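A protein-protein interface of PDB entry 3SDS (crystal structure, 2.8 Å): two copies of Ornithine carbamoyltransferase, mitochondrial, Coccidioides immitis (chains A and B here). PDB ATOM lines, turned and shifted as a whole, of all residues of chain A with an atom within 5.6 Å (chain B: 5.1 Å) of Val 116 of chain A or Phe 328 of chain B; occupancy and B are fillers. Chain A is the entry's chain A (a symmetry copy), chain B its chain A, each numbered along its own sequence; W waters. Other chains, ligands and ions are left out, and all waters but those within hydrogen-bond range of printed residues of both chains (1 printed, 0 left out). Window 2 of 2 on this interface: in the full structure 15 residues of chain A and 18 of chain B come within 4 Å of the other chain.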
ATOM      1  N   LEU A 111      -5.329   2.056  -1.010  1.00  0.00           N
ATOM      2  CA  LEU A 111      -6.741   1.959  -1.468  1.00  0.00           C
ATOM      3  C   LEU A 111      -7.565   3.233  -1.171  1.00  0.00           C
ATOM      4  O   LEU A 111      -8.489   3.591  -1.920  1.00  0.00           O
ATOM      5  CB  LEU A 111      -7.462   0.695  -0.954  1.00  0.00           C
ATOM      6  CG  LEU A 111      -8.854   0.506  -1.604  1.00  0.00           C
ATOM      7  CD1 LEU A 111      -9.083  -0.895  -2.179  1.00  0.00           C
ATOM      8  CD2 LEU A 111     -10.013   0.920  -0.684  1.00  0.00           C
ATOM      9  N   TYR A 112      -7.211   3.899  -0.070  1.00  0.00           N
ATOM     10  CA  TYR A 112      -7.832   5.157   0.314  1.00  0.00           C
ATOM     11  C   TYR A 112      -7.689   6.197  -0.814  1.00  0.00           C
ATOM     12  O   TYR A 112      -8.698   6.704  -1.323  1.00  0.00           O
ATOM     13  CB  TYR A 112      -7.211   5.643   1.625  1.00  0.00           C
ATOM     14  CG  TYR A 112      -7.897   6.832   2.255  1.00  0.00           C
ATOM     15  CD1 TYR A 112      -9.090   6.681   2.972  1.00  0.00           C
ATOM     16  CD2 TYR A 112      -7.340   8.114   2.156  1.00  0.00           C
ATOM     17  CE1 TYR A 112      -9.712   7.772   3.565  1.00  0.00           C
ATOM     18  CE2 TYR A 112      -7.960   9.215   2.747  1.00  0.00           C
ATOM     19  CZ  TYR A 112      -9.144   9.031   3.451  1.00  0.00           C
ATOM     20  OH  TYR A 112      -9.753  10.113   4.028  1.00  0.00           O
ATOM     21  N   ASP A 113      -6.440   6.458  -1.212  1.00  0.00           N
ATOM     22  CA  ASP A 113      -6.094   7.439  -2.241  1.00  0.00           C
ATOM     23  C   ASP A 113      -6.832   7.216  -3.585  1.00  0.00           C
ATOM     24  O   ASP A 113      -7.536   8.107  -4.087  1.00  0.00           O
ATOM     25  CB  ASP A 113      -4.575   7.445  -2.464  1.00  0.00           C
ATOM     26  CG  ASP A 113      -3.777   7.862  -1.218  1.00  0.00           C
ATOM     27  OD1 ASP A 113      -4.341   7.913  -0.100  1.00  0.00           O
ATOM     28  OD2 ASP A 113      -2.562   8.149  -1.362  1.00  0.00           O
ATOM     29  N   THR A 114      -6.681   6.021  -4.151  1.00  0.00           N
ATOM     30  CA  THR A 114      -7.358   5.648  -5.392  1.00  0.00           C
ATOM     31  C   THR A 114      -8.864   5.954  -5.358  1.00  0.00           C
ATOM     32  O   THR A 114      -9.423   6.563  -6.275  1.00  0.00           O
ATOM     33  CB  THR A 114      -7.116   4.163  -5.666  1.00  0.00           C
ATOM     34  OG1 THR A 114      -5.734   3.985  -5.993  1.00  0.00           O
ATOM     35  CG2 THR A 114      -7.971   3.653  -6.808  1.00  0.00           C
ATOM     36  N   SER A 115      -9.497   5.522  -4.277  1.00  0.00           N
ATOM     37  CA  SER A 115     -10.903   5.760  -3.984  1.00  0.00           C
ATOM     38  C   SER A 115     -11.307   7.258  -3.943  1.00  0.00           C
ATOM     39  O   SER A 115     -12.286   7.644  -4.557  1.00  0.00           O
ATOM     40  CB  SER A 115     -11.218   5.087  -2.652  1.00  0.00           C
ATOM     41  OG  SER A 115     -12.599   4.881  -2.511  1.00  0.00           O
ATOM     42  N   VAL A 116     -10.562   8.098  -3.225  1.00  0.00           N
ATOM     43  CA  VAL A 116     -10.936   9.506  -3.122  1.00  0.00           C
ATOM     44  C   VAL A 116     -10.772  10.195  -4.477  1.00  0.00           C
ATOM     45  O   VAL A 116     -11.693  10.897  -4.935  1.00  0.00           O
ATOM     46  CB  VAL A 116     -10.149  10.253  -2.017  1.00  0.00           C
ATOM     47  CG1 VAL A 116     -10.151  11.779  -2.254  1.00  0.00           C
ATOM     48  CG2 VAL A 116     -10.699   9.914  -0.640  1.00  0.00           C
ATOM     49  N   VAL A 117      -9.622   9.943  -5.117  1.00  0.00           N
ATOM     50  CA  VAL A 117      -9.215  10.561  -6.393  1.00  0.00           C
ATOM     51  C   VAL A 117     -10.103  10.238  -7.604  1.00  0.00           C
ATOM     52  O   VAL A 117     -10.558  11.148  -8.299  1.00  0.00           O
ATOM     53  CB  VAL A 117      -7.726  10.241  -6.717  1.00  0.00           C
ATOM     54  CG1 VAL A 117      -7.308  10.822  -8.079  1.00  0.00           C
ATOM     55  CG2 VAL A 117      -6.832  10.795  -5.623  1.00  0.00           C
ATOM     56  N   ILE A 118     -10.337   8.955  -7.869  1.00  0.00           N
ATOM     57  CA  ILE A 118     -11.182   8.553  -9.008  1.00  0.00           C
ATOM     58  C   ILE A 118     -12.611   9.039  -8.833  1.00  0.00           C
ATOM     59  O   ILE A 118     -13.186   9.603  -9.772  1.00  0.00           O
ATOM     60  CB  ILE A 118     -11.144   7.018  -9.290  1.00  0.00           C
ATOM     61  CG1 ILE A 118      -9.716   6.603  -9.670  1.00  0.00           C
ATOM     62  CG2 ILE A 118     -12.094   6.638 -10.413  1.00  0.00           C
ATOM     63  CD1 ILE A 118      -9.568   5.184 -10.222  1.00  0.00           C
ATOM     64  N   SER A 119     -13.164   8.856  -7.632  1.00  0.00           N
ATOM     65  CA  SER A 119     -14.552   9.254  -7.364  1.00  0.00           C
ATOM     66  C   SER A 119     -14.794  10.768  -7.496  1.00  0.00           C
ATOM     67  O   SER A 119     -15.936  11.199  -7.715  1.00  0.00           O
ATOM     68  CB  SER A 119     -15.050   8.726  -6.003  1.00  0.00           C
ATOM     69  OG  SER A 119     -14.521   9.455  -4.927  1.00  0.00           O
ATOM     70  N   SER A 120     -13.734  11.569  -7.382  1.00  0.00           N
ATOM     71  CA  SER A 120     -13.896  13.008  -7.487  1.00  0.00           C
ATOM     72  C   SER A 120     -14.008  13.518  -8.940  1.00  0.00           C
ATOM     73  O   SER A 120     -14.376  14.682  -9.170  1.00  0.00           O
ATOM     74  CB  SER A 120     -12.821  13.751  -6.674  1.00  0.00           C
ATOM     75  OG  SER A 120     -11.522  13.610  -7.219  1.00  0.00           O
ATOM     76  N   HIS A 141     -14.996   5.170   1.159  1.00  0.00           N
ATOM     77  CA  HIS A 141     -14.364   6.456   0.869  1.00  0.00           C
ATOM     78  C   HIS A 141     -14.706   7.090  -0.495  1.00  0.00           C
ATOM     79  O   HIS A 141     -14.168   8.134  -0.842  1.00  0.00           O
ATOM     80  CB  HIS A 141     -12.851   6.333   1.062  1.00  0.00           C
ATOM     81  CG  HIS A 141     -12.461   5.718   2.374  1.00  0.00           C
ATOM     82  ND1 HIS A 141     -12.053   4.403   2.489  1.00  0.00           N
ATOM     83  CD2 HIS A 141     -12.437   6.231   3.629  1.00  0.00           C
ATOM     84  CE1 HIS A 141     -11.781   4.136   3.755  1.00  0.00           C
ATOM     85  NE2 HIS A 141     -12.002   5.229   4.465  1.00  0.00           N
ATOM     86  N   SER A 143     -16.960   9.266  -2.982  1.00  0.00           N
ATOM     87  CA  SER A 143     -17.961  10.322  -2.875  1.00  0.00           C
ATOM     88  C   SER A 143     -19.111  10.182  -3.877  1.00  0.00           C
ATOM     89  O   SER A 143     -19.991  11.046  -3.928  1.00  0.00           O
ATOM     90  CB  SER A 143     -17.324  11.697  -2.978  1.00  0.00           C
ATOM     91  OG  SER A 143     -16.658  11.815  -4.206  1.00  0.00           O
ATOM     92  N   PHE B 320       1.168  14.130   5.134  1.00  0.00           N
ATOM     93  CA  PHE B 320       0.323  13.816   3.967  1.00  0.00           C
ATOM     94  C   PHE B 320      -1.155  13.990   4.274  1.00  0.00           C
ATOM     95  O   PHE B 320      -1.899  14.511   3.442  1.00  0.00           O
ATOM     96  CB  PHE B 320       0.603  12.382   3.474  1.00  0.00           C
ATOM     97  CG  PHE B 320       0.059  12.072   2.091  1.00  0.00           C
ATOM     98  CD1 PHE B 320       0.622  12.657   0.947  1.00  0.00           C
ATOM     99  CD2 PHE B 320      -0.990  11.159   1.932  1.00  0.00           C
ATOM    100  CE1 PHE B 320       0.131  12.355  -0.339  1.00  0.00           C
ATOM    101  CE2 PHE B 320      -1.487  10.848   0.651  1.00  0.00           C
ATOM    102  CZ  PHE B 320      -0.932  11.450  -0.490  1.00  0.00           C
ATOM    103  N   TYR B 321      -1.562  13.575   5.476  1.00  0.00           N
ATOM    104  CA  TYR B 321      -2.973  13.554   5.850  1.00  0.00           C
ATOM    105  C   TYR B 321      -3.415  14.700   6.755  1.00  0.00           C
ATOM    106  O   TYR B 321      -4.577  14.742   7.157  1.00  0.00           O
ATOM    107  CB  TYR B 321      -3.358  12.208   6.481  1.00  0.00           C
ATOM    108  CG  TYR B 321      -3.305  11.039   5.522  1.00  0.00           C
ATOM    109  CD1 TYR B 321      -4.133  10.994   4.409  1.00  0.00           C
ATOM    110  CD2 TYR B 321      -2.422   9.974   5.735  1.00  0.00           C
ATOM    111  CE1 TYR B 321      -4.091   9.927   3.537  1.00  0.00           C
ATOM    112  CE2 TYR B 321      -2.368   8.899   4.854  1.00  0.00           C
ATOM    113  CZ  TYR B 321      -3.210   8.883   3.761  1.00  0.00           C
ATOM    114  OH  TYR B 321      -3.184   7.830   2.883  1.00  0.00           O
ATOM    115  N   LEU B 326      -2.905  19.767   0.400  1.00  0.00           N
ATOM    116  CA  LEU B 326      -3.802  20.118  -0.707  1.00  0.00           C
ATOM    117  C   LEU B 326      -3.814  19.038  -1.814  1.00  0.00           C
ATOM    118  O   LEU B 326      -4.330  19.254  -2.929  1.00  0.00           O
ATOM    119  CB  LEU B 326      -3.399  21.465  -1.304  1.00  0.00           C
ATOM    120  CG  LEU B 326      -3.190  22.668  -0.394  1.00  0.00           C
ATOM    121  CD1 LEU B 326      -2.590  23.815  -1.221  1.00  0.00           C
ATOM    122  CD2 LEU B 326      -4.496  23.078   0.259  1.00  0.00           C
ATOM    123  N   VAL B 327      -3.243  17.883  -1.466  1.00  0.00           N
ATOM    124  CA  VAL B 327      -3.068  16.721  -2.331  1.00  0.00           C
ATOM    125  C   VAL B 327      -4.306  16.281  -3.175  1.00  0.00           C
ATOM    126  O   VAL B 327      -4.210  16.150  -4.405  1.00  0.00           O
ATOM    127  CB  VAL B 327      -2.444  15.565  -1.487  1.00  0.00           C
ATOM    128  CG1 VAL B 327      -3.022  14.205  -1.847  1.00  0.00           C
ATOM    129  CG2 VAL B 327      -0.940  15.585  -1.614  1.00  0.00           C
ATOM    130  N   PHE B 328      -5.453  16.076  -2.536  1.00  0.00           N
ATOM    131  CA  PHE B 328      -6.656  15.618  -3.249  1.00  0.00           C
ATOM    132  C   PHE B 328      -7.326  16.714  -4.117  1.00  0.00           C
ATOM    133  O   PHE B 328      -7.678  16.472  -5.289  1.00  0.00           O
ATOM    134  CB  PHE B 328      -7.646  14.953  -2.275  1.00  0.00           C
ATOM    135  CG  PHE B 328      -7.061  13.772  -1.537  1.00  0.00           C
ATOM    136  CD1 PHE B 328      -6.787  12.572  -2.210  1.00  0.00           C
ATOM    137  CD2 PHE B 328      -6.746  13.866  -0.181  1.00  0.00           C
ATOM    138  CE1 PHE B 328      -6.228  11.476  -1.538  1.00  0.00           C
ATOM    139  CE2 PHE B 328      -6.173  12.785   0.499  1.00  0.00           C
ATOM    140  CZ  PHE B 328      -5.921  11.582  -0.182  1.00  0.00           C
ATOM    141  N   PRO B 329      -7.501  17.927  -3.563  1.00  0.00           N
ATOM    142  CA  PRO B 329      -7.944  18.982  -4.483  1.00  0.00           C
ATOM    143  C   PRO B 329      -7.022  19.136  -5.707  1.00  0.00           C
ATOM    144  O   PRO B 329      -7.523  19.306  -6.823  1.00  0.00           O
ATOM    145  CB  PRO B 329      -7.918  20.236  -3.601  1.00  0.00           C
ATOM    146  CG  PRO B 329      -8.248  19.691  -2.228  1.00  0.00           C
ATOM    147  CD  PRO B 329      -7.493  18.393  -2.162  1.00  0.00           C
ATOM    148  N   GLU B 330      -5.703  19.049  -5.492  1.00  0.00           N
ATOM    149  CA  GLU B 330      -4.702  19.148  -6.559  1.00  0.00           C
ATOM    150  C   GLU B 330      -4.888  18.058  -7.618  1.00  0.00           C
ATOM    151  O   GLU B 330      -4.726  18.314  -8.816  1.00  0.00           O
ATOM    152  CB  GLU B 330      -3.302  19.039  -5.959  1.00  0.00           C
ATOM    153  CG  GLU B 330      -2.176  19.253  -6.955  1.00  0.00           C
ATOM    154  CD  GLU B 330      -0.791  18.942  -6.395  1.00  0.00           C
ATOM    155  OE1 GLU B 330      -0.676  18.558  -5.205  1.00  0.00           O
ATOM    156  OE2 GLU B 330       0.197  19.080  -7.163  1.00  0.00           O
ATOM    157  N   ALA B 331      -5.221  16.844  -7.164  1.00  0.00           N
ATOM    158  CA  ALA B 331      -5.494  15.711  -8.059  1.00  0.00           C
ATOM    159  C   ALA B 331      -6.741  15.951  -8.934  1.00  0.00           C
ATOM    160  O   ALA B 331      -6.699  15.738 -10.142  1.00  0.00           O
ATOM    161  CB  ALA B 331      -5.614  14.414  -7.255  1.00  0.00           C
ATOM    162  N   GLU B 332      -7.833  16.399  -8.308  1.00  0.00           N
ATOM    163  CA  GLU B 332      -9.078  16.766  -8.999  1.00  0.00           C
ATOM    164  C   GLU B 332      -8.929  17.952  -9.967  1.00  0.00           C
ATOM    165  O   GLU B 332      -9.610  17.994 -11.014  1.00  0.00           O
ATOM    166  CB  GLU B 332     -10.203  17.061  -7.989  1.00  0.00           C
ATOM    167  CG  GLU B 332     -11.495  17.610  -8.625  1.00  0.00           C
ATOM    168  CD  GLU B 332     -12.505  18.171  -7.642  1.00  0.00           C
ATOM    169  OE1 GLU B 332     -12.476  17.820  -6.438  1.00  0.00           O
ATOM    170  OE2 GLU B 332     -13.349  18.974  -8.087  1.00  0.00           O
ATOM    171  N   ASN B 333      -8.064  18.912  -9.633  1.00  0.00           N
ATOM    172  CA  ASN B 333      -7.850  20.050 -10.527  1.00  0.00           C
ATOM    173  C   ASN B 333      -7.262  19.664 -11.904  1.00  0.00           C
ATOM    174  O   ASN B 333      -7.163  20.515 -12.796  1.00  0.00           O
ATOM    175  CB  ASN B 333      -7.015  21.139  -9.844  1.00  0.00           C
ATOM    176  CG  ASN B 333      -7.779  21.870  -8.707  1.00  0.00           C
ATOM    177  OD1 ASN B 333      -9.017  21.931  -8.689  1.00  0.00           O
ATOM    178  ND2 ASN B 333      -7.025  22.435  -7.762  1.00  0.00           N
HETATM  179  O   HOH W   1      -9.296  14.331  -5.206  1.00  0.00           O
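The side-chain hydroxyl of Tyr 321 of chain B lies within hydrogen-bond range of the side-chain carboxylate of Asp 113 of chain A (3.2 Å).
The backbone carbonyl oxygen of Val 116 of chain A lies within hydrogen-bond range of the side-chain hydroxyl of Ser 119 of chain A, at 3.2 Å.
The backbone carbonyl oxygen of Val 117 of chain A sits at hydrogen-bond distance from the side-chain hydroxyl of Ser 120 of chain A.
CD2 of Tyr 112 of chain A touches CE1 of Tyr 321 of chain B, at 3.97 Å.
Phe 320 of chain B touches Asp 113 of chain A.
Phe 328 of chain B touches Asp 113 of chain A.
CD1 of Phe 328 of chain B touches CG1 of Val 116 of chain A (3.5 Å).
Val 117 of chain A touches Phe 328 of chain B (CG2 to CD1, 3.8 Å).
Glu 332 of chain B touches Ser 120 of chain A.
Leu 111 of chain A touches none of the printed residues of chain B.
Printed residues of chain B within 4 Å of Tyr 112 of chain A: Tyr 321 (3.97 Å).
Val 116 of chain A touches just one residue of chain B: Phe 328 (3.5 Å).
Printed residues of chain A within 4 Å of Tyr 321 of chain B: Tyr 112 (3.97 Å) and Asp 113 (3.2 Å).
Printed residues of chain A within 4 Å of Phe 328 of chain B: Asp 113, Val 116 and Val 117.
Asn 333 of chain B touches none of the printed residues of chain A.
The nearest printed residue of chain B that does not touch Val 116 of chain A is Pro 329 of chain B (6.8 Å).
The nearest printed residue of chain A that does not touch Glu 332 of chain B is Val 117 of chain A (5.6 Å).
Printed residues of chain B that touch a printed residue of chain A: Phe 320, Tyr 321, Phe 328 and Glu 332.
Hydrophobic or aromatic side chains of chain B that line the printed part of chain A: Phe 320, Tyr 321 and Phe 328.
Printed residues of chain A that touch a printed residue of chain B: Tyr 112, Asp 113, Val 116, Val 117 and Ser 120.
Hydrophobic or aromatic side chains of chain A within 4 Å of the printed part of chain B: Tyr 112, Val 116 and Val 117.
Along chain A the printed residues that touch a printed residue of chain B span positions 112 to 120.
Among the printed residues, 7 pairs touch across the chains.
No position is printed for both chains.
Of the 7 pairs that touch across the chains among the printed residues, none has its exchanged pair printed and touching as well.
Water W1 lies within hydrogen-bond range of O of Phe 328 of chain B (2.7 Å) and OG of Ser 120 of chain A (3.1 Å).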
